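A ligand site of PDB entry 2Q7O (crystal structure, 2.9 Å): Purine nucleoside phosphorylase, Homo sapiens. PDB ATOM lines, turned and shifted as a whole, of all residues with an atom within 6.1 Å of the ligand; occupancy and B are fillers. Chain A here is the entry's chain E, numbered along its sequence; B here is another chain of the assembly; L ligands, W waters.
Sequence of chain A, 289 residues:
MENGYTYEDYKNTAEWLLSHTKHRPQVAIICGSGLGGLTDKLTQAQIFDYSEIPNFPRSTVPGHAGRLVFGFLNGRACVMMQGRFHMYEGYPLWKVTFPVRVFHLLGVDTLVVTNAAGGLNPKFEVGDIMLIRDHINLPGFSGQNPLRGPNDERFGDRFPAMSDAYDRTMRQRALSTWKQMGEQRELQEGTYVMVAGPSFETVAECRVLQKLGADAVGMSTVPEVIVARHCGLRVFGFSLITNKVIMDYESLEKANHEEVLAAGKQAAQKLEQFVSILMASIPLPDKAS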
ATOM      1  N   GLY A  32     -23.283   3.331  -7.692  1.00  0.00           N
ATOM      2  CA  GLY A  32     -22.274   4.371  -7.334  1.00  0.00           C
ATOM      3  C   GLY A  32     -22.714   5.774  -7.835  1.00  0.00           C
ATOM      4  O   GLY A  32     -22.326   6.787  -7.219  1.00  0.00           O
ATOM      5  N   SER A  33     -23.348   5.894  -9.028  1.00  0.00           N
ATOM      6  CA  SER A  33     -22.968   5.125 -10.251  1.00  0.00           C
ATOM      7  C   SER A  33     -21.484   5.467 -10.533  1.00  0.00           C
ATOM      8  O   SER A  33     -20.650   4.567 -10.615  1.00  0.00           O
ATOM      9  CB  SER A  33     -23.832   5.499 -11.465  1.00  0.00           C
ATOM     10  OG  SER A  33     -23.827   6.901 -11.710  1.00  0.00           O
ATOM     11  N   HIS A  86     -33.589   1.292  -8.824  1.00  0.00           N
ATOM     12  CA  HIS A  86     -34.222   2.193  -7.876  1.00  0.00           C
ATOM     13  C   HIS A  86     -35.719   2.096  -7.869  1.00  0.00           C
ATOM     14  O   HIS A  86     -36.367   1.664  -8.829  1.00  0.00           O
ATOM     15  CB  HIS A  86     -33.848   3.626  -8.115  1.00  0.00           C
ATOM     16  CG  HIS A  86     -32.404   3.830  -8.410  1.00  0.00           C
ATOM     17  ND1 HIS A  86     -31.730   4.965  -8.045  1.00  0.00           N
ATOM     18  CD2 HIS A  86     -31.514   3.059  -9.062  1.00  0.00           C
ATOM     19  CE1 HIS A  86     -30.493   4.897  -8.476  1.00  0.00           C
ATOM     20  NE2 HIS A  86     -30.337   3.736  -9.090  1.00  0.00           N
ATOM     21  N   TYR A  88     -37.585   4.720  -7.620  1.00  0.00           N
ATOM     22  CA  TYR A  88     -38.241   5.718  -8.363  1.00  0.00           C
ATOM     23  C   TYR A  88     -38.369   5.256  -9.794  1.00  0.00           C
ATOM     24  O   TYR A  88     -39.213   5.779 -10.485  1.00  0.00           O
ATOM     25  CB  TYR A  88     -37.550   7.068  -8.261  1.00  0.00           C
ATOM     26  CG  TYR A  88     -36.147   7.064  -8.737  1.00  0.00           C
ATOM     27  CD1 TYR A  88     -35.096   7.126  -7.831  1.00  0.00           C
ATOM     28  CD2 TYR A  88     -35.831   7.010 -10.096  1.00  0.00           C
ATOM     29  CE1 TYR A  88     -33.820   7.150  -8.236  1.00  0.00           C
ATOM     30  CE2 TYR A  88     -34.493   7.002 -10.504  1.00  0.00           C
ATOM     31  CZ  TYR A  88     -33.515   7.071  -9.552  1.00  0.00           C
ATOM     32  OH  TYR A  88     -32.229   7.091  -9.929  1.00  0.00           O
ATOM     33  N   ASN A 115     -22.772   5.188  -2.817  1.00  0.00           N
ATOM     34  CA  ASN A 115     -23.807   5.941  -3.438  1.00  0.00           C
ATOM     35  C   ASN A 115     -23.528   7.417  -3.374  1.00  0.00           C
ATOM     36  O   ASN A 115     -22.760   7.872  -2.499  1.00  0.00           O
ATOM     37  CB  ASN A 115     -25.171   5.675  -2.781  1.00  0.00           C
ATOM     38  CG  ASN A 115     -25.324   6.291  -1.353  1.00  0.00           C
ATOM     39  OD1 ASN A 115     -25.520   5.585  -0.400  1.00  0.00           O
ATOM     40  ND2 ASN A 115     -25.339   7.587  -1.243  1.00  0.00           N
ATOM     41  N   ALA A 116     -24.145   8.223  -4.241  1.00  0.00           N
ATOM     42  CA  ALA A 116     -24.065   9.688  -4.016  1.00  0.00           C
ATOM     43  C   ALA A 116     -25.213  10.112  -3.157  1.00  0.00           C
ATOM     44  O   ALA A 116     -26.184   9.380  -2.986  1.00  0.00           O
ATOM     45  CB  ALA A 116     -24.072  10.499  -5.303  1.00  0.00           C
ATOM     46  N   ALA A 117     -25.133  11.323  -2.628  1.00  0.00           N
ATOM     47  CA  ALA A 117     -26.114  11.799  -1.688  1.00  0.00           C
ATOM     48  C   ALA A 117     -25.968  13.261  -1.466  1.00  0.00           C
ATOM     49  O   ALA A 117     -24.889  13.868  -1.581  1.00  0.00           O
ATOM     50  CB  ALA A 117     -25.947  11.097  -0.382  1.00  0.00           C
ATOM     51  N   GLY A 118     -27.068  13.884  -1.135  1.00  0.00           N
ATOM     52  CA  GLY A 118     -26.999  15.271  -0.803  1.00  0.00           C
ATOM     53  C   GLY A 118     -26.575  15.411   0.631  1.00  0.00           C
ATOM     54  O   GLY A 118     -26.822  14.536   1.473  1.00  0.00           O
ATOM     55  N   GLY A 119     -25.963  16.522   0.950  1.00  0.00           N
ATOM     56  CA  GLY A 119     -25.518  16.713   2.297  1.00  0.00           C
ATOM     57  C   GLY A 119     -26.509  17.562   3.019  1.00  0.00           C
ATOM     58  O   GLY A 119     -26.968  18.584   2.498  1.00  0.00           O
ATOM     59  N   TYR A 192     -27.587   8.090   6.804  1.00  0.00           N
ATOM     60  CA  TYR A 192     -28.236   8.261   5.484  1.00  0.00           C
ATOM     61  C   TYR A 192     -29.756   8.119   5.691  1.00  0.00           C
ATOM     62  O   TYR A 192     -30.226   7.095   6.207  1.00  0.00           O
ATOM     63  CB  TYR A 192     -27.709   7.224   4.528  1.00  0.00           C
ATOM     64  CG  TYR A 192     -28.277   7.174   3.104  1.00  0.00           C
ATOM     65  CD1 TYR A 192     -27.617   7.805   2.059  1.00  0.00           C
ATOM     66  CD2 TYR A 192     -29.411   6.425   2.811  1.00  0.00           C
ATOM     67  CE1 TYR A 192     -28.117   7.722   0.729  1.00  0.00           C
ATOM     68  CE2 TYR A 192     -29.898   6.344   1.488  1.00  0.00           C
ATOM     69  CZ  TYR A 192     -29.247   6.979   0.457  1.00  0.00           C
ATOM     70  OH  TYR A 192     -29.722   6.830  -0.825  1.00  0.00           O
ATOM     71  N   VAL A 195     -35.318   8.958   1.057  1.00  0.00           N
ATOM     72  CA  VAL A 195     -36.626   9.127   0.415  1.00  0.00           C
ATOM     73  C   VAL A 195     -36.616   8.561  -0.997  1.00  0.00           C
ATOM     74  O   VAL A 195     -35.562   8.424  -1.615  1.00  0.00           O
ATOM     75  CB  VAL A 195     -37.055  10.602   0.382  1.00  0.00           C
ATOM     76  CG1 VAL A 195     -36.550  11.332   1.613  1.00  0.00           C
ATOM     77  CG2 VAL A 195     -36.550  11.266  -0.888  1.00  0.00           C
ATOM     78  N   PRO A 198     -38.435  10.659  -7.631  1.00  0.00           N
ATOM     79  CA  PRO A 198     -37.187  11.107  -8.245  1.00  0.00           C
ATOM     80  C   PRO A 198     -36.976  12.614  -8.070  1.00  0.00           C
ATOM     81  O   PRO A 198     -35.850  13.099  -8.231  1.00  0.00           O
ATOM     82  CB  PRO A 198     -37.387  10.776  -9.729  1.00  0.00           C
ATOM     83  CG  PRO A 198     -38.859  10.836  -9.921  1.00  0.00           C
ATOM     84  CD  PRO A 198     -39.465  10.345  -8.638  1.00  0.00           C
ATOM     85  N   SER A 199     -38.049  13.334  -7.754  1.00  0.00           N
ATOM     86  CA  SER A 199     -37.979  14.746  -7.607  1.00  0.00           C
ATOM     87  C   SER A 199     -37.013  15.138  -6.475  1.00  0.00           C
ATOM     88  O   SER A 199     -36.928  14.387  -5.533  1.00  0.00           O
ATOM     89  CB  SER A 199     -39.432  15.206  -7.402  1.00  0.00           C
ATOM     90  OG  SER A 199     -39.745  15.458  -6.036  1.00  0.00           O
ATOM     91  N   PHE A 200     -36.276  16.251  -6.546  1.00  0.00           N
ATOM     92  CA  PHE A 200     -35.376  16.628  -5.439  1.00  0.00           C
ATOM     93  C   PHE A 200     -36.185  17.329  -4.374  1.00  0.00           C
ATOM     94  O   PHE A 200     -37.282  17.797  -4.674  1.00  0.00           O
ATOM     95  CB  PHE A 200     -34.259  17.581  -5.860  1.00  0.00           C
ATOM     96  CG  PHE A 200     -33.128  16.914  -6.576  1.00  0.00           C
ATOM     97  CD1 PHE A 200     -32.141  16.229  -5.860  1.00  0.00           C
ATOM     98  CD2 PHE A 200     -33.021  16.984  -7.979  1.00  0.00           C
ATOM     99  CE1 PHE A 200     -31.065  15.601  -6.523  1.00  0.00           C
ATOM    100  CE2 PHE A 200     -31.967  16.358  -8.662  1.00  0.00           C
ATOM    101  CZ  PHE A 200     -30.980  15.650  -7.924  1.00  0.00           C
ATOM    102  N   GLU A 201     -35.649  17.453  -3.175  1.00  0.00           N
ATOM    103  CA  GLU A 201     -36.444  17.870  -2.019  1.00  0.00           C
ATOM    104  C   GLU A 201     -36.708  19.338  -2.077  1.00  0.00           C
ATOM    105  O   GLU A 201     -35.940  20.077  -2.669  1.00  0.00           O
ATOM    106  CB  GLU A 201     -35.693  17.589  -0.699  1.00  0.00           C
ATOM    107  CG  GLU A 201     -35.363  16.133  -0.411  1.00  0.00           C
ATOM    108  CD  GLU A 201     -34.391  15.524  -1.443  1.00  0.00           C
ATOM    109  OE1 GLU A 201     -34.789  14.522  -2.137  1.00  0.00           O
ATOM    110  OE2 GLU A 201     -33.266  16.090  -1.575  1.00  0.00           O
ATOM    111  N   VAL A 217     -28.682  12.402   2.235  1.00  0.00           N
ATOM    112  CA  VAL A 217     -29.955  11.939   1.667  1.00  0.00           C
ATOM    113  C   VAL A 217     -29.901  11.391   0.260  1.00  0.00           C
ATOM    114  O   VAL A 217     -29.611  12.121  -0.663  1.00  0.00           O
ATOM    115  CB  VAL A 217     -30.996  13.074   1.734  1.00  0.00           C
ATOM    116  CG1 VAL A 217     -30.504  14.337   1.020  1.00  0.00           C
ATOM    117  CG2 VAL A 217     -32.273  12.606   1.146  1.00  0.00           C
ATOM    118  N   GLY A 218     -30.212  10.104   0.085  1.00  0.00           N
ATOM    119  CA  GLY A 218     -30.353   9.570  -1.289  1.00  0.00           C
ATOM    120  C   GLY A 218     -31.688   8.890  -1.407  1.00  0.00           C
ATOM    121  O   GLY A 218     -32.396   8.843  -0.414  1.00  0.00           O
ATOM    122  N   MET A 219     -31.875   8.236  -2.530  1.00  0.00           N
ATOM    123  CA  MET A 219     -33.065   7.538  -2.883  1.00  0.00           C
ATOM    124  C   MET A 219     -32.723   6.094  -3.050  1.00  0.00           C
ATOM    125  O   MET A 219     -33.372   5.398  -3.798  1.00  0.00           O
ATOM    126  CB  MET A 219     -33.563   8.085  -4.204  1.00  0.00           C
ATOM    127  CG  MET A 219     -33.393   9.566  -4.289  1.00  0.00           C
ATOM    128  SD  MET A 219     -34.062  10.359  -5.713  1.00  0.00           S
ATOM    129  CE  MET A 219     -34.107  12.025  -5.196  1.00  0.00           C
ATOM    130  N   SER A 220     -31.695   5.619  -2.342  1.00  0.00           N
ATOM    131  CA  SER A 220     -31.017   4.369  -2.720  1.00  0.00           C
ATOM    132  C   SER A 220     -30.601   3.486  -1.529  1.00  0.00           C
ATOM    133  O   SER A 220     -30.762   3.883  -0.378  1.00  0.00           O
ATOM    134  CB  SER A 220     -29.795   4.671  -3.595  1.00  0.00           C
ATOM    135  OG  SER A 220     -28.599   4.225  -2.976  1.00  0.00           O
ATOM    136  N   THR A 242     -22.196  15.535  -2.658  1.00  0.00           N
ATOM    137  CA  THR A 242     -22.246  15.654  -4.078  1.00  0.00           C
ATOM    138  C   THR A 242     -22.957  16.942  -4.343  1.00  0.00           C
ATOM    139  O   THR A 242     -22.925  17.459  -5.442  1.00  0.00           O
ATOM    140  CB  THR A 242     -23.016  14.484  -4.607  1.00  0.00           C
ATOM    141  OG1 THR A 242     -22.334  13.959  -5.749  1.00  0.00           O
ATOM    142  CG2 THR A 242     -24.427  14.834  -4.966  1.00  0.00           C
ATOM    143  N   ASN A 243     -23.599  17.468  -3.296  1.00  0.00           N
ATOM    144  CA  ASN A 243     -24.229  18.752  -3.339  1.00  0.00           C
ATOM    145  C   ASN A 243     -24.707  19.035  -1.956  1.00  0.00           C
ATOM    146  O   ASN A 243     -25.038  18.120  -1.236  1.00  0.00           O
ATOM    147  CB  ASN A 243     -25.398  18.798  -4.322  1.00  0.00           C
ATOM    148  CG  ASN A 243     -26.461  17.766  -4.018  1.00  0.00           C
ATOM    149  OD1 ASN A 243     -26.256  16.561  -4.197  1.00  0.00           O
ATOM    150  ND2 ASN A 243     -27.600  18.231  -3.521  1.00  0.00           N
ATOM    151  N   LYS A 244     -24.683  20.310  -1.586  1.00  0.00           N
ATOM    152  CA  LYS A 244     -25.224  20.789  -0.332  1.00  0.00           C
ATOM    153  C   LYS A 244     -26.676  21.115  -0.617  1.00  0.00           C
ATOM    154  O   LYS A 244     -26.999  22.018  -1.396  1.00  0.00           O
ATOM    155  CB  LYS A 244     -24.485  22.030   0.178  1.00  0.00           C
ATOM    156  CG  LYS A 244     -23.155  21.758   0.945  1.00  0.00           C
ATOM    157  CD  LYS A 244     -22.406  23.132   1.242  1.00  0.00           C
ATOM    158  CE  LYS A 244     -21.379  23.071   2.446  1.00  0.00           C
ATOM    159  NZ  LYS A 244     -21.907  23.451   3.826  1.00  0.00           N
ATOM    160  N   VAL A 245     -27.545  20.333  -0.020  1.00  0.00           N
ATOM    161  CA  VAL A 245     -28.955  20.455  -0.258  1.00  0.00           C
ATOM    162  C   VAL A 245     -29.403  21.864   0.113  1.00  0.00           C
ATOM    163  O   VAL A 245     -29.111  22.335   1.201  1.00  0.00           O
ATOM    164  CB  VAL A 245     -29.653  19.391   0.547  1.00  0.00           C
ATOM    165  CG1 VAL A 245     -31.069  19.327   0.132  1.00  0.00           C
ATOM    166  CG2 VAL A 245     -28.994  18.050   0.248  1.00  0.00           C
ATOM    167  N   ALA A 255     -30.568  21.830  -6.957  1.00  0.00           N
ATOM    168  CA  ALA A 255     -29.923  20.538  -7.163  1.00  0.00           C
ATOM    169  C   ALA A 255     -30.166  20.119  -8.615  1.00  0.00           C
ATOM    170  O   ALA A 255     -31.243  20.306  -9.136  1.00  0.00           O
ATOM    171  CB  ALA A 255     -30.503  19.536  -6.244  1.00  0.00           C
ATOM    172  N   HIS A 257     -28.352  16.989 -11.767  1.00  0.00           N
ATOM    173  CA  HIS A 257     -27.885  15.613 -11.771  1.00  0.00           C
ATOM    174  C   HIS A 257     -26.602  15.462 -12.587  1.00  0.00           C
ATOM    175  O   HIS A 257     -25.713  14.698 -12.226  1.00  0.00           O
ATOM    176  CB  HIS A 257     -28.964  14.675 -12.316  1.00  0.00           C
ATOM    177  CG  HIS A 257     -28.589  13.228 -12.278  1.00  0.00           C
ATOM    178  ND1 HIS A 257     -28.305  12.504 -13.417  1.00  0.00           N
ATOM    179  CD2 HIS A 257     -28.442  12.369 -11.241  1.00  0.00           C
ATOM    180  CE1 HIS A 257     -27.997  11.260 -13.092  1.00  0.00           C
ATOM    181  NE2 HIS A 257     -28.074  11.148 -11.770  1.00  0.00           N
ATOM    182  N   VAL A 260     -24.368  16.440 -10.010  1.00  0.00           N
ATOM    183  CA  VAL A 260     -24.152  15.209  -9.268  1.00  0.00           C
ATOM    184  C   VAL A 260     -23.203  14.325 -10.009  1.00  0.00           C
ATOM    185  O   VAL A 260     -22.220  13.909  -9.433  1.00  0.00           O
ATOM    186  CB  VAL A 260     -25.448  14.442  -8.935  1.00  0.00           C
ATOM    187  CG1 VAL A 260     -25.129  13.074  -8.299  1.00  0.00           C
ATOM    188  CG2 VAL A 260     -26.330  15.281  -8.014  1.00  0.00           C
ATOM    189  N   PHE B 159     -35.091  14.207 -12.909  1.00  0.00           N
ATOM    190  CA  PHE B 159     -34.681  14.608 -11.530  1.00  0.00           C
ATOM    191  C   PHE B 159     -34.880  16.123 -11.302  1.00  0.00           C
ATOM    192  O   PHE B 159     -33.927  16.824 -10.983  1.00  0.00           O
ATOM    193  CB  PHE B 159     -33.176  14.272 -11.220  1.00  0.00           C
ATOM    194  CG  PHE B 159     -32.860  12.816 -11.158  1.00  0.00           C
ATOM    195  CD1 PHE B 159     -33.544  11.986 -10.282  1.00  0.00           C
ATOM    196  CD2 PHE B 159     -31.868  12.283 -11.979  1.00  0.00           C
ATOM    197  CE1 PHE B 159     -33.255  10.609 -10.232  1.00  0.00           C
ATOM    198  CE2 PHE B 159     -31.561  10.919 -11.937  1.00  0.00           C
ATOM    199  CZ  PHE B 159     -32.279  10.068 -11.052  1.00  0.00           C
HETATM  200  O1  LIG L   1     -31.124  12.509  -7.434  1.00  0.00           O
HETATM  201  C1  LIG L   1     -30.199  11.803  -8.250  1.00  0.00           C
HETATM  202  C2  LIG L   1     -29.855  10.611  -7.410  1.00  0.00           C
HETATM  203  N1  LIG L   1     -30.033  10.787  -5.961  1.00  0.00           N
HETATM  204  C3  LIG L   1     -28.395  10.507  -7.593  1.00  0.00           C
HETATM  205  O2  LIG L   1     -28.268   9.255  -8.284  1.00  0.00           O
HETATM  206  C4  LIG L   1     -27.758  10.560  -6.180  1.00  0.00           C
HETATM  207  O3  LIG L   1     -27.075   9.320  -5.857  1.00  0.00           O
HETATM  208  C5  LIG L   1     -28.821  10.866  -5.143  1.00  0.00           C
HETATM  209  C6  LIG L   1     -28.731  12.253  -4.663  1.00  0.00           C
HETATM  210  C7  LIG L   1     -27.689  13.124  -4.853  1.00  0.00           C
HETATM  211  N2  LIG L   1     -28.046  14.317  -4.290  1.00  0.00           N
HETATM  212  C8  LIG L   1     -29.258  14.270  -3.754  1.00  0.00           C
HETATM  213  C9  LIG L   1     -30.129  15.200  -3.054  1.00  0.00           C
HETATM  214  O4  LIG L   1     -29.701  16.467  -2.836  1.00  0.00           O
HETATM  215  N3  LIG L   1     -31.338  14.742  -2.654  1.00  0.00           N
HETATM  216  C10 LIG L   1     -31.753  13.483  -2.901  1.00  0.00           C
HETATM  217  N4  LIG L   1     -31.024  12.556  -3.557  1.00  0.00           N
HETATM  218  C11 LIG L   1     -29.809  12.940  -3.964  1.00  0.00           C
HETATM  219  O   HOH W   1     -26.478   6.553  -6.587  1.00  0.00           O
HETATM  220  O   HOH W   2     -31.430  18.437  -2.866  1.00  0.00           O
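Water W2 bridges an oxygen (O4) of the ligand (2.6 Å) and the side-chain carboxylate (OE2) of Glu 201 (3.2 Å).
The backbone carbonyl oxygen (O) of Val 217 sits close to a nitrogen (N4) of the ligand (3.2 Å).
A nitrogen (N2) of the ligand lies close to the backbone NH (N) of Gly 118, 3.3 Å away.
An oxygen (O4) of the ligand lies within hydrogen-bond range of the side-chain amide nitrogen of Asn 243 (2.8 Å).
The backbone carbonyl oxygen (O) of Ala 116 lies within hydrogen-bond range of an oxygen (O3) of the ligand (3.0 Å).
OE2 of Glu 201 lies within hydrogen-bond range of N3 of the ligand, at 2.6 Å.
O of Asn 243 sits at hydrogen-bond distance from N of Gly 119, 2.9 Å away.
N of Val 195 is in hydrogen-bond range of O of Gly 218 (3.3 Å).
The backbone NH (N) of Val 217 sits at hydrogen-bond distance from the backbone carbonyl oxygen (O) of Gly 118 (2.9 Å).
O of Gly 218 lies close to OH of Tyr 192 (3.4 Å).
The backbone carbonyl oxygen (O) of Ala 117 lies within hydrogen-bond range of the backbone NH (N) of Thr 242 (3.3 Å).
OH of Tyr 192 lies within hydrogen-bond range of N of Met 219 (3.1 Å).
O of Gly 119 sits close to N of Val 245, 3.1 Å away.
C of Ala 117 touches N2 of the ligand, at 3.7 Å.
Phe 200 touches the ligand.
Gly 218 touches the ligand (CA to N4, 3.8 Å).
Met 219 touches the ligand (CE to N4, 3.5 Å).
CG2 of Thr 242 touches C7 of the ligand (3.7 Å).
Val 245 touches the ligand.
CD2 of His 257 touches C1 of the ligand (3.5 Å).
CD1 of Phe 159 of chain B touches O1 of the ligand (3.8 Å).
The nearest printed residue that does not touch the ligand is Val 260 (4.1 Å).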
